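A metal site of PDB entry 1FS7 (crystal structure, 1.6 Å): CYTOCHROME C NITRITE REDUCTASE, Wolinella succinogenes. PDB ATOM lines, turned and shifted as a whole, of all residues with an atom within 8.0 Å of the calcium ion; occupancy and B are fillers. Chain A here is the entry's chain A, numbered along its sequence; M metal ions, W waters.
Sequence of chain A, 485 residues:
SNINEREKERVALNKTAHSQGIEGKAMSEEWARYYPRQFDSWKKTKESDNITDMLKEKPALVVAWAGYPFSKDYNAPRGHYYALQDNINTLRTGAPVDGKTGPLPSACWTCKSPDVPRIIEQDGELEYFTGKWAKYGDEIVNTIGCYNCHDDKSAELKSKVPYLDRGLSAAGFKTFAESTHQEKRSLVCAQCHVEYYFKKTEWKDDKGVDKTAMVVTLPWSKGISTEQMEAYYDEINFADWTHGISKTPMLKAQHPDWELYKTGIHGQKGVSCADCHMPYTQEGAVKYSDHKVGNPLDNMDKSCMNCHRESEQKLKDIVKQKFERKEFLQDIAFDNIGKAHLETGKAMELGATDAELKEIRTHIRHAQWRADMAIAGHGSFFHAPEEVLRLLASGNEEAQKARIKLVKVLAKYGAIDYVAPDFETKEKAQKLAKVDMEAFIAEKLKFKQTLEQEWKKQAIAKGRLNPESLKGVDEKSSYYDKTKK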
ATOM      1  N   TYR A  68      38.986  16.497 -28.120  1.00  0.00           N
ATOM      2  CA  TYR A  68      38.222  17.338 -27.193  1.00  0.00           C
ATOM      3  C   TYR A  68      39.010  17.512 -25.885  1.00  0.00           C
ATOM      4  O   TYR A  68      39.796  16.653 -25.503  1.00  0.00           O
ATOM      5  CB  TYR A  68      36.870  16.658 -26.920  1.00  0.00           C
ATOM      6  CG  TYR A  68      35.742  17.575 -26.506  1.00  0.00           C
ATOM      7  CD1 TYR A  68      35.404  18.684 -27.283  1.00  0.00           C
ATOM      8  CD2 TYR A  68      35.002  17.309 -25.365  1.00  0.00           C
ATOM      9  CE1 TYR A  68      34.349  19.519 -26.917  1.00  0.00           C
ATOM     10  CE2 TYR A  68      33.939  18.137 -24.990  1.00  0.00           C
ATOM     11  CZ  TYR A  68      33.623  19.227 -25.775  1.00  0.00           C
ATOM     12  OH  TYR A  68      32.576  20.037 -25.399  1.00  0.00           O
ATOM     13  N   VAL A 194      23.318  19.476 -14.019  1.00  0.00           N
ATOM     14  CA  VAL A 194      22.525  19.093 -15.182  1.00  0.00           C
ATOM     15  C   VAL A 194      23.371  19.081 -16.450  1.00  0.00           C
ATOM     16  O   VAL A 194      24.504  19.571 -16.451  1.00  0.00           O
ATOM     17  CB  VAL A 194      21.360  20.098 -15.412  1.00  0.00           C
ATOM     18  CG1 VAL A 194      20.327  19.975 -14.304  1.00  0.00           C
ATOM     19  CG2 VAL A 194      21.913  21.513 -15.464  1.00  0.00           C
ATOM     20  N   GLU A 195      22.831  18.507 -17.521  1.00  0.00           N
ATOM     21  CA  GLU A 195      23.516  18.459 -18.807  1.00  0.00           C
ATOM     22  C   GLU A 195      23.240  19.793 -19.486  1.00  0.00           C
ATOM     23  O   GLU A 195      22.171  20.384 -19.292  1.00  0.00           O
ATOM     24  CB  GLU A 195      23.000  17.281 -19.657  1.00  0.00           C
ATOM     25  CG  GLU A 195      22.886  17.522 -21.164  1.00  0.00           C
ATOM     26  CD  GLU A 195      24.224  17.729 -21.870  1.00  0.00           C
ATOM     27  OE1 GLU A 195      25.284  17.574 -21.245  1.00  0.00           O
ATOM     28  OE2 GLU A 195      24.198  18.028 -23.080  1.00  0.00           O
ATOM     29  N   TYR A 196      24.196  20.271 -20.286  1.00  0.00           N
ATOM     30  CA  TYR A 196      24.041  21.559 -20.950  1.00  0.00           C
ATOM     31  C   TYR A 196      24.895  21.620 -22.206  1.00  0.00           C
ATOM     32  O   TYR A 196      25.670  20.710 -22.494  1.00  0.00           O
ATOM     33  CB  TYR A 196      24.517  22.679 -20.028  1.00  0.00           C
ATOM     34  CG  TYR A 196      26.037  22.703 -19.902  1.00  0.00           C
ATOM     35  CD1 TYR A 196      26.708  21.800 -19.066  1.00  0.00           C
ATOM     36  CD2 TYR A 196      26.800  23.555 -20.698  1.00  0.00           C
ATOM     37  CE1 TYR A 196      28.102  21.742 -19.045  1.00  0.00           C
ATOM     38  CE2 TYR A 196      28.194  23.497 -20.678  1.00  0.00           C
ATOM     39  CZ  TYR A 196      28.841  22.592 -19.865  1.00  0.00           C
ATOM     40  OH  TYR A 196      30.222  22.516 -19.894  1.00  0.00           O
ATOM     41  N   TYR A 197      24.749  22.710 -22.948  1.00  0.00           N
ATOM     42  CA  TYR A 197      25.573  22.954 -24.122  1.00  0.00           C
ATOM     43  C   TYR A 197      25.630  24.459 -24.310  1.00  0.00           C
ATOM     44  O   TYR A 197      24.769  25.180 -23.809  1.00  0.00           O
ATOM     45  CB  TYR A 197      25.023  22.252 -25.378  1.00  0.00           C
ATOM     46  CG  TYR A 197      23.883  22.972 -26.072  1.00  0.00           C
ATOM     47  CD1 TYR A 197      22.574  22.835 -25.618  1.00  0.00           C
ATOM     48  CD2 TYR A 197      24.113  23.752 -27.208  1.00  0.00           C
ATOM     49  CE1 TYR A 197      21.525  23.457 -26.280  1.00  0.00           C
ATOM     50  CE2 TYR A 197      23.068  24.372 -27.879  1.00  0.00           C
ATOM     51  CZ  TYR A 197      21.768  24.222 -27.406  1.00  0.00           C
ATOM     52  OH  TYR A 197      20.721  24.811 -28.071  1.00  0.00           O
ATOM     53  N   PHE A 198      26.672  24.950 -24.978  1.00  0.00           N
ATOM     54  CA  PHE A 198      26.795  26.386 -25.198  1.00  0.00           C
ATOM     55  C   PHE A 198      26.159  26.764 -26.522  1.00  0.00           C
ATOM     56  O   PHE A 198      26.525  26.232 -27.571  1.00  0.00           O
ATOM     57  CB  PHE A 198      28.268  26.821 -25.230  1.00  0.00           C
ATOM     58  CG  PHE A 198      29.005  26.618 -23.926  1.00  0.00           C
ATOM     59  CD1 PHE A 198      28.357  26.769 -22.700  1.00  0.00           C
ATOM     60  CD2 PHE A 198      30.372  26.346 -23.931  1.00  0.00           C
ATOM     61  CE1 PHE A 198      29.055  26.653 -21.503  1.00  0.00           C
ATOM     62  CE2 PHE A 198      31.083  26.225 -22.737  1.00  0.00           C
ATOM     63  CZ  PHE A 198      30.418  26.382 -21.522  1.00  0.00           C
ATOM     64  N   THR A 217      22.792  26.485 -22.094  1.00  0.00           N
ATOM     65  CA  THR A 217      21.441  26.103 -22.480  1.00  0.00           C
ATOM     66  C   THR A 217      21.183  24.645 -22.130  1.00  0.00           C
ATOM     67  O   THR A 217      21.989  23.777 -22.445  1.00  0.00           O
ATOM     68  CB  THR A 217      21.245  26.267 -24.001  1.00  0.00           C
ATOM     69  OG1 THR A 217      21.635  27.589 -24.391  1.00  0.00           O
ATOM     70  CG2 THR A 217      19.792  26.010 -24.385  1.00  0.00           C
ATOM     71  N   PRO A 219      19.388  21.365 -22.893  1.00  0.00           N
ATOM     72  CA  PRO A 219      18.750  20.721 -24.046  1.00  0.00           C
ATOM     73  C   PRO A 219      17.467  19.973 -23.665  1.00  0.00           C
ATOM     74  O   PRO A 219      17.306  18.798 -24.001  1.00  0.00           O
ATOM     75  CB  PRO A 219      19.833  19.766 -24.532  1.00  0.00           C
ATOM     76  CG  PRO A 219      20.406  19.283 -23.229  1.00  0.00           C
ATOM     77  CD  PRO A 219      20.540  20.572 -22.428  1.00  0.00           C
ATOM     78  N   MET A 229      16.809  14.264 -25.488  1.00  0.00           N
ATOM     79  CA  MET A 229      17.901  15.216 -25.667  1.00  0.00           C
ATOM     80  C   MET A 229      18.655  14.896 -26.951  1.00  0.00           C
ATOM     81  O   MET A 229      19.097  15.796 -27.670  1.00  0.00           O
ATOM     82  CB  MET A 229      18.854  15.143 -24.462  1.00  0.00           C
ATOM     83  CG  MET A 229      18.225  15.629 -23.161  1.00  0.00           C
ATOM     84  SD  MET A 229      19.451  15.883 -21.862  1.00  0.00           S
ATOM     85  CE  MET A 229      18.910  14.751 -20.628  1.00  0.00           C
ATOM     86  N   TYR A 233      19.436  17.464 -30.061  1.00  0.00           N
ATOM     87  CA  TYR A 233      20.716  17.780 -30.683  1.00  0.00           C
ATOM     88  C   TYR A 233      20.750  17.430 -32.171  1.00  0.00           C
ATOM     89  O   TYR A 233      21.353  18.150 -32.965  1.00  0.00           O
ATOM     90  CB  TYR A 233      21.858  17.060 -29.953  1.00  0.00           C
ATOM     91  CG  TYR A 233      22.218  17.696 -28.621  1.00  0.00           C
ATOM     92  CD1 TYR A 233      22.670  19.013 -28.566  1.00  0.00           C
ATOM     93  CD2 TYR A 233      22.126  16.971 -27.437  1.00  0.00           C
ATOM     94  CE1 TYR A 233      23.008  19.602 -27.350  1.00  0.00           C
ATOM     95  CE2 TYR A 233      22.467  17.559 -26.208  1.00  0.00           C
ATOM     96  CZ  TYR A 233      22.908  18.868 -26.180  1.00  0.00           C
ATOM     97  OH  TYR A 233      23.242  19.459 -24.977  1.00  0.00           O
ATOM     98  N   PHE A 238      23.573  19.640 -34.154  1.00  0.00           N
ATOM     99  CA  PHE A 238      24.606  20.109 -33.241  1.00  0.00           C
ATOM    100  C   PHE A 238      25.693  19.071 -32.941  1.00  0.00           C
ATOM    101  O   PHE A 238      25.429  17.878 -32.868  1.00  0.00           O
ATOM    102  CB  PHE A 238      23.971  20.545 -31.921  1.00  0.00           C
ATOM    103  CG  PHE A 238      24.952  21.110 -30.941  1.00  0.00           C
ATOM    104  CD1 PHE A 238      25.369  22.437 -31.044  1.00  0.00           C
ATOM    105  CD2 PHE A 238      25.487  20.326 -29.925  1.00  0.00           C
ATOM    106  CE1 PHE A 238      26.301  22.965 -30.149  1.00  0.00           C
ATOM    107  CE2 PHE A 238      26.417  20.845 -29.031  1.00  0.00           C
ATOM    108  CZ  PHE A 238      26.822  22.154 -29.147  1.00  0.00           C
ATOM    109  N   ASP A 240      29.388  18.901 -30.394  1.00  0.00           N
ATOM    110  CA  ASP A 240      30.274  19.587 -29.466  1.00  0.00           C
ATOM    111  C   ASP A 240      31.683  19.630 -30.066  1.00  0.00           C
ATOM    112  O   ASP A 240      32.438  20.578 -29.822  1.00  0.00           O
ATOM    113  CB  ASP A 240      30.279  18.860 -28.117  1.00  0.00           C
ATOM    114  CG  ASP A 240      29.030  19.167 -27.303  1.00  0.00           C
ATOM    115  OD1 ASP A 240      28.874  20.315 -26.862  1.00  0.00           O
ATOM    116  OD2 ASP A 240      28.198  18.245 -27.112  1.00  0.00           O
ATOM    117  N   LEU A 251      28.733  14.406 -29.452  1.00  0.00           N
ATOM    118  CA  LEU A 251      27.955  15.073 -28.426  1.00  0.00           C
ATOM    119  C   LEU A 251      28.585  14.708 -27.085  1.00  0.00           C
ATOM    120  O   LEU A 251      28.845  13.533 -26.815  1.00  0.00           O
ATOM    121  CB  LEU A 251      26.493  14.600 -28.437  1.00  0.00           C
ATOM    122  CG  LEU A 251      25.653  14.930 -29.673  1.00  0.00           C
ATOM    123  CD1 LEU A 251      24.275  14.289 -29.559  1.00  0.00           C
ATOM    124  CD2 LEU A 251      25.533  16.438 -29.828  1.00  0.00           C
ATOM    125  N   LYS A 252      28.825  15.712 -26.248  1.00  0.00           N
ATOM    126  CA  LYS A 252      29.415  15.490 -24.935  1.00  0.00           C
ATOM    127  C   LYS A 252      28.360  15.611 -23.844  1.00  0.00           C
ATOM    128  O   LYS A 252      27.671  16.633 -23.753  1.00  0.00           O
ATOM    129  CB  LYS A 252      30.511  16.523 -24.660  1.00  0.00           C
ATOM    130  CG  LYS A 252      31.214  16.323 -23.316  1.00  0.00           C
ATOM    131  CD  LYS A 252      32.177  15.144 -23.370  1.00  0.00           C
ATOM    132  CE  LYS A 252      32.713  14.773 -21.996  1.00  0.00           C
ATOM    133  NZ  LYS A 252      31.725  14.039 -21.157  1.00  0.00           N
ATOM    134  N   ALA A 253      28.232  14.594 -23.006  1.00  0.00           N
ATOM    135  CA  ALA A 253      27.286  14.662 -21.905  1.00  0.00           C
ATOM    136  C   ALA A 253      28.061  15.192 -20.703  1.00  0.00           C
ATOM    137  O   ALA A 253      29.217  14.831 -20.511  1.00  0.00           O
ATOM    138  CB  ALA A 253      26.722  13.288 -21.582  1.00  0.00           C
ATOM    139  N   GLN A 254      27.435  16.053 -19.915  1.00  0.00           N
ATOM    140  CA  GLN A 254      28.076  16.569 -18.722  1.00  0.00           C
ATOM    141  C   GLN A 254      27.154  16.470 -17.539  1.00  0.00           C
ATOM    142  O   GLN A 254      26.053  17.037 -17.552  1.00  0.00           O
ATOM    143  CB  GLN A 254      28.516  18.026 -18.887  1.00  0.00           C
ATOM    144  CG  GLN A 254      29.699  18.223 -19.831  1.00  0.00           C
ATOM    145  CD  GLN A 254      29.285  18.838 -21.137  1.00  0.00           C
ATOM    146  OE1 GLN A 254      28.152  18.672 -21.571  1.00  0.00           O
ATOM    147  NE2 GLN A 254      30.198  19.550 -21.780  1.00  0.00           N
ATOM    148  N   HIS A 255      27.586  15.714 -16.537  1.00  0.00           N
ATOM    149  CA  HIS A 255      26.849  15.556 -15.291  1.00  0.00           C
ATOM    150  C   HIS A 255      25.341  15.818 -15.322  1.00  0.00           C
ATOM    151  O   HIS A 255      24.862  16.822 -14.776  1.00  0.00           O
ATOM    152  CB  HIS A 255      27.500  16.451 -14.231  1.00  0.00           C
ATOM    153  CG  HIS A 255      27.922  17.790 -14.746  1.00  0.00           C
ATOM    154  ND1 HIS A 255      27.022  18.711 -15.246  1.00  0.00           N
ATOM    155  CD2 HIS A 255      29.151  18.348 -14.907  1.00  0.00           C
ATOM    156  CE1 HIS A 255      27.674  19.772 -15.686  1.00  0.00           C
ATOM    157  NE2 HIS A 255      28.964  19.574 -15.494  1.00  0.00           N
ATOM    158  N   TRP A 369      26.804   9.117 -27.004  1.00  0.00           N
ATOM    159  CA  TRP A 369      25.912  10.045 -26.322  1.00  0.00           C
ATOM    160  C   TRP A 369      25.169   9.299 -25.206  1.00  0.00           C
ATOM    161  O   TRP A 369      25.090   9.777 -24.078  1.00  0.00           O
ATOM    162  CB  TRP A 369      24.885  10.653 -27.278  1.00  0.00           C
ATOM    163  CG  TRP A 369      23.789  11.413 -26.562  1.00  0.00           C
ATOM    164  CD1 TRP A 369      22.469  11.071 -26.483  1.00  0.00           C
ATOM    165  CD2 TRP A 369      23.951  12.597 -25.770  1.00  0.00           C
ATOM    166  NE1 TRP A 369      21.796  11.972 -25.693  1.00  0.00           N
ATOM    167  CE2 TRP A 369      22.682  12.916 -25.244  1.00  0.00           C
ATOM    168  CE3 TRP A 369      25.038  13.409 -25.452  1.00  0.00           C
ATOM    169  CZ2 TRP A 369      22.478  14.025 -24.417  1.00  0.00           C
ATOM    170  CZ3 TRP A 369      24.834  14.517 -24.626  1.00  0.00           C
ATOM    171  CH2 TRP A 369      23.556  14.808 -24.121  1.00  0.00           C
ATOM    172  N   ASP A 372      27.774   8.027 -22.493  1.00  0.00           N
ATOM    173  CA  ASP A 372      28.282   9.174 -21.732  1.00  0.00           C
ATOM    174  C   ASP A 372      27.177   9.685 -20.808  1.00  0.00           C
ATOM    175  O   ASP A 372      27.430   9.995 -19.644  1.00  0.00           O
ATOM    176  CB  ASP A 372      28.749  10.285 -22.691  1.00  0.00           C
ATOM    177  CG  ASP A 372      29.803  11.201 -22.068  1.00  0.00           C
ATOM    178  OD1 ASP A 372      30.258  10.952 -20.934  1.00  0.00           O
ATOM    179  OD2 ASP A 372      30.186  12.177 -22.744  1.00  0.00           O
ATOM    180  N   MET A 373      25.945   9.769 -21.311  1.00  0.00           N
ATOM    181  CA  MET A 373      24.829  10.239 -20.475  1.00  0.00           C
ATOM    182  C   MET A 373      24.642   9.316 -19.275  1.00  0.00           C
ATOM    183  O   MET A 373      24.204   9.747 -18.208  1.00  0.00           O
ATOM    184  CB  MET A 373      23.524  10.293 -21.285  1.00  0.00           C
ATOM    185  CG  MET A 373      23.292  11.608 -22.029  1.00  0.00           C
ATOM    186  SD  MET A 373      23.084  13.023 -20.903  1.00  0.00           S
ATOM    187  CE  MET A 373      21.531  12.610 -20.127  1.00  0.00           C
HETATM  188 CA    CA M   1      26.579  18.673 -23.216  1.00  0.00          CA
HETATM  189  O   HOH W   1      28.188  20.129 -24.301  1.00  0.00           O
HETATM  190  O   HOH W   2      26.115  18.624 -25.609  1.00  0.00           O
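OD2 of Asp 240 is in hydrogen-bond range of N of Lys 252 (2.7 Å). The backbone NH of Phe 238 is in hydrogen-bond range of the backbone carbonyl oxygen of Tyr 233, 2.9 Å away. The side-chain carboxylate of Glu 195 sits close to the side-chain hydroxyl of Tyr 233, at 2.6 Å. OD2 of Asp 372 is in salt-bridge range of NZ of Lys 252 (2.9 Å).
Merely in contact with the calcium ion: Tyr 233. Five residues have an atom within 4 Å of the calcium ion: Glu 195, Tyr 196, Tyr 233, Lys 252 and Gln 254.
The calcium ion is bound by OE1 of Gln 254, 2.3 Å away. O of Tyr 196 binds the calcium ion. The calcium ion is bound by O of Lys 252, at 2.4 Å. Water W1 binds the calcium ion (2.4 Å). Water W2 is bound to the calcium ion (2.4 Å). The calcium ion is bound by OE2 of Glu 195, 2.5 Å away. The side-chain carboxylate (OE1) of Glu 195 binds the calcium ion.
Water W2 lies within hydrogen-bond range of OD2 of Asp 240 and OH of Tyr 233. Water W1 lies within hydrogen-bond range of the side-chain carboxylate of Asp 240 (2.7 Å) and the side-chain amide nitrogen of Gln 254 (3.3 Å).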
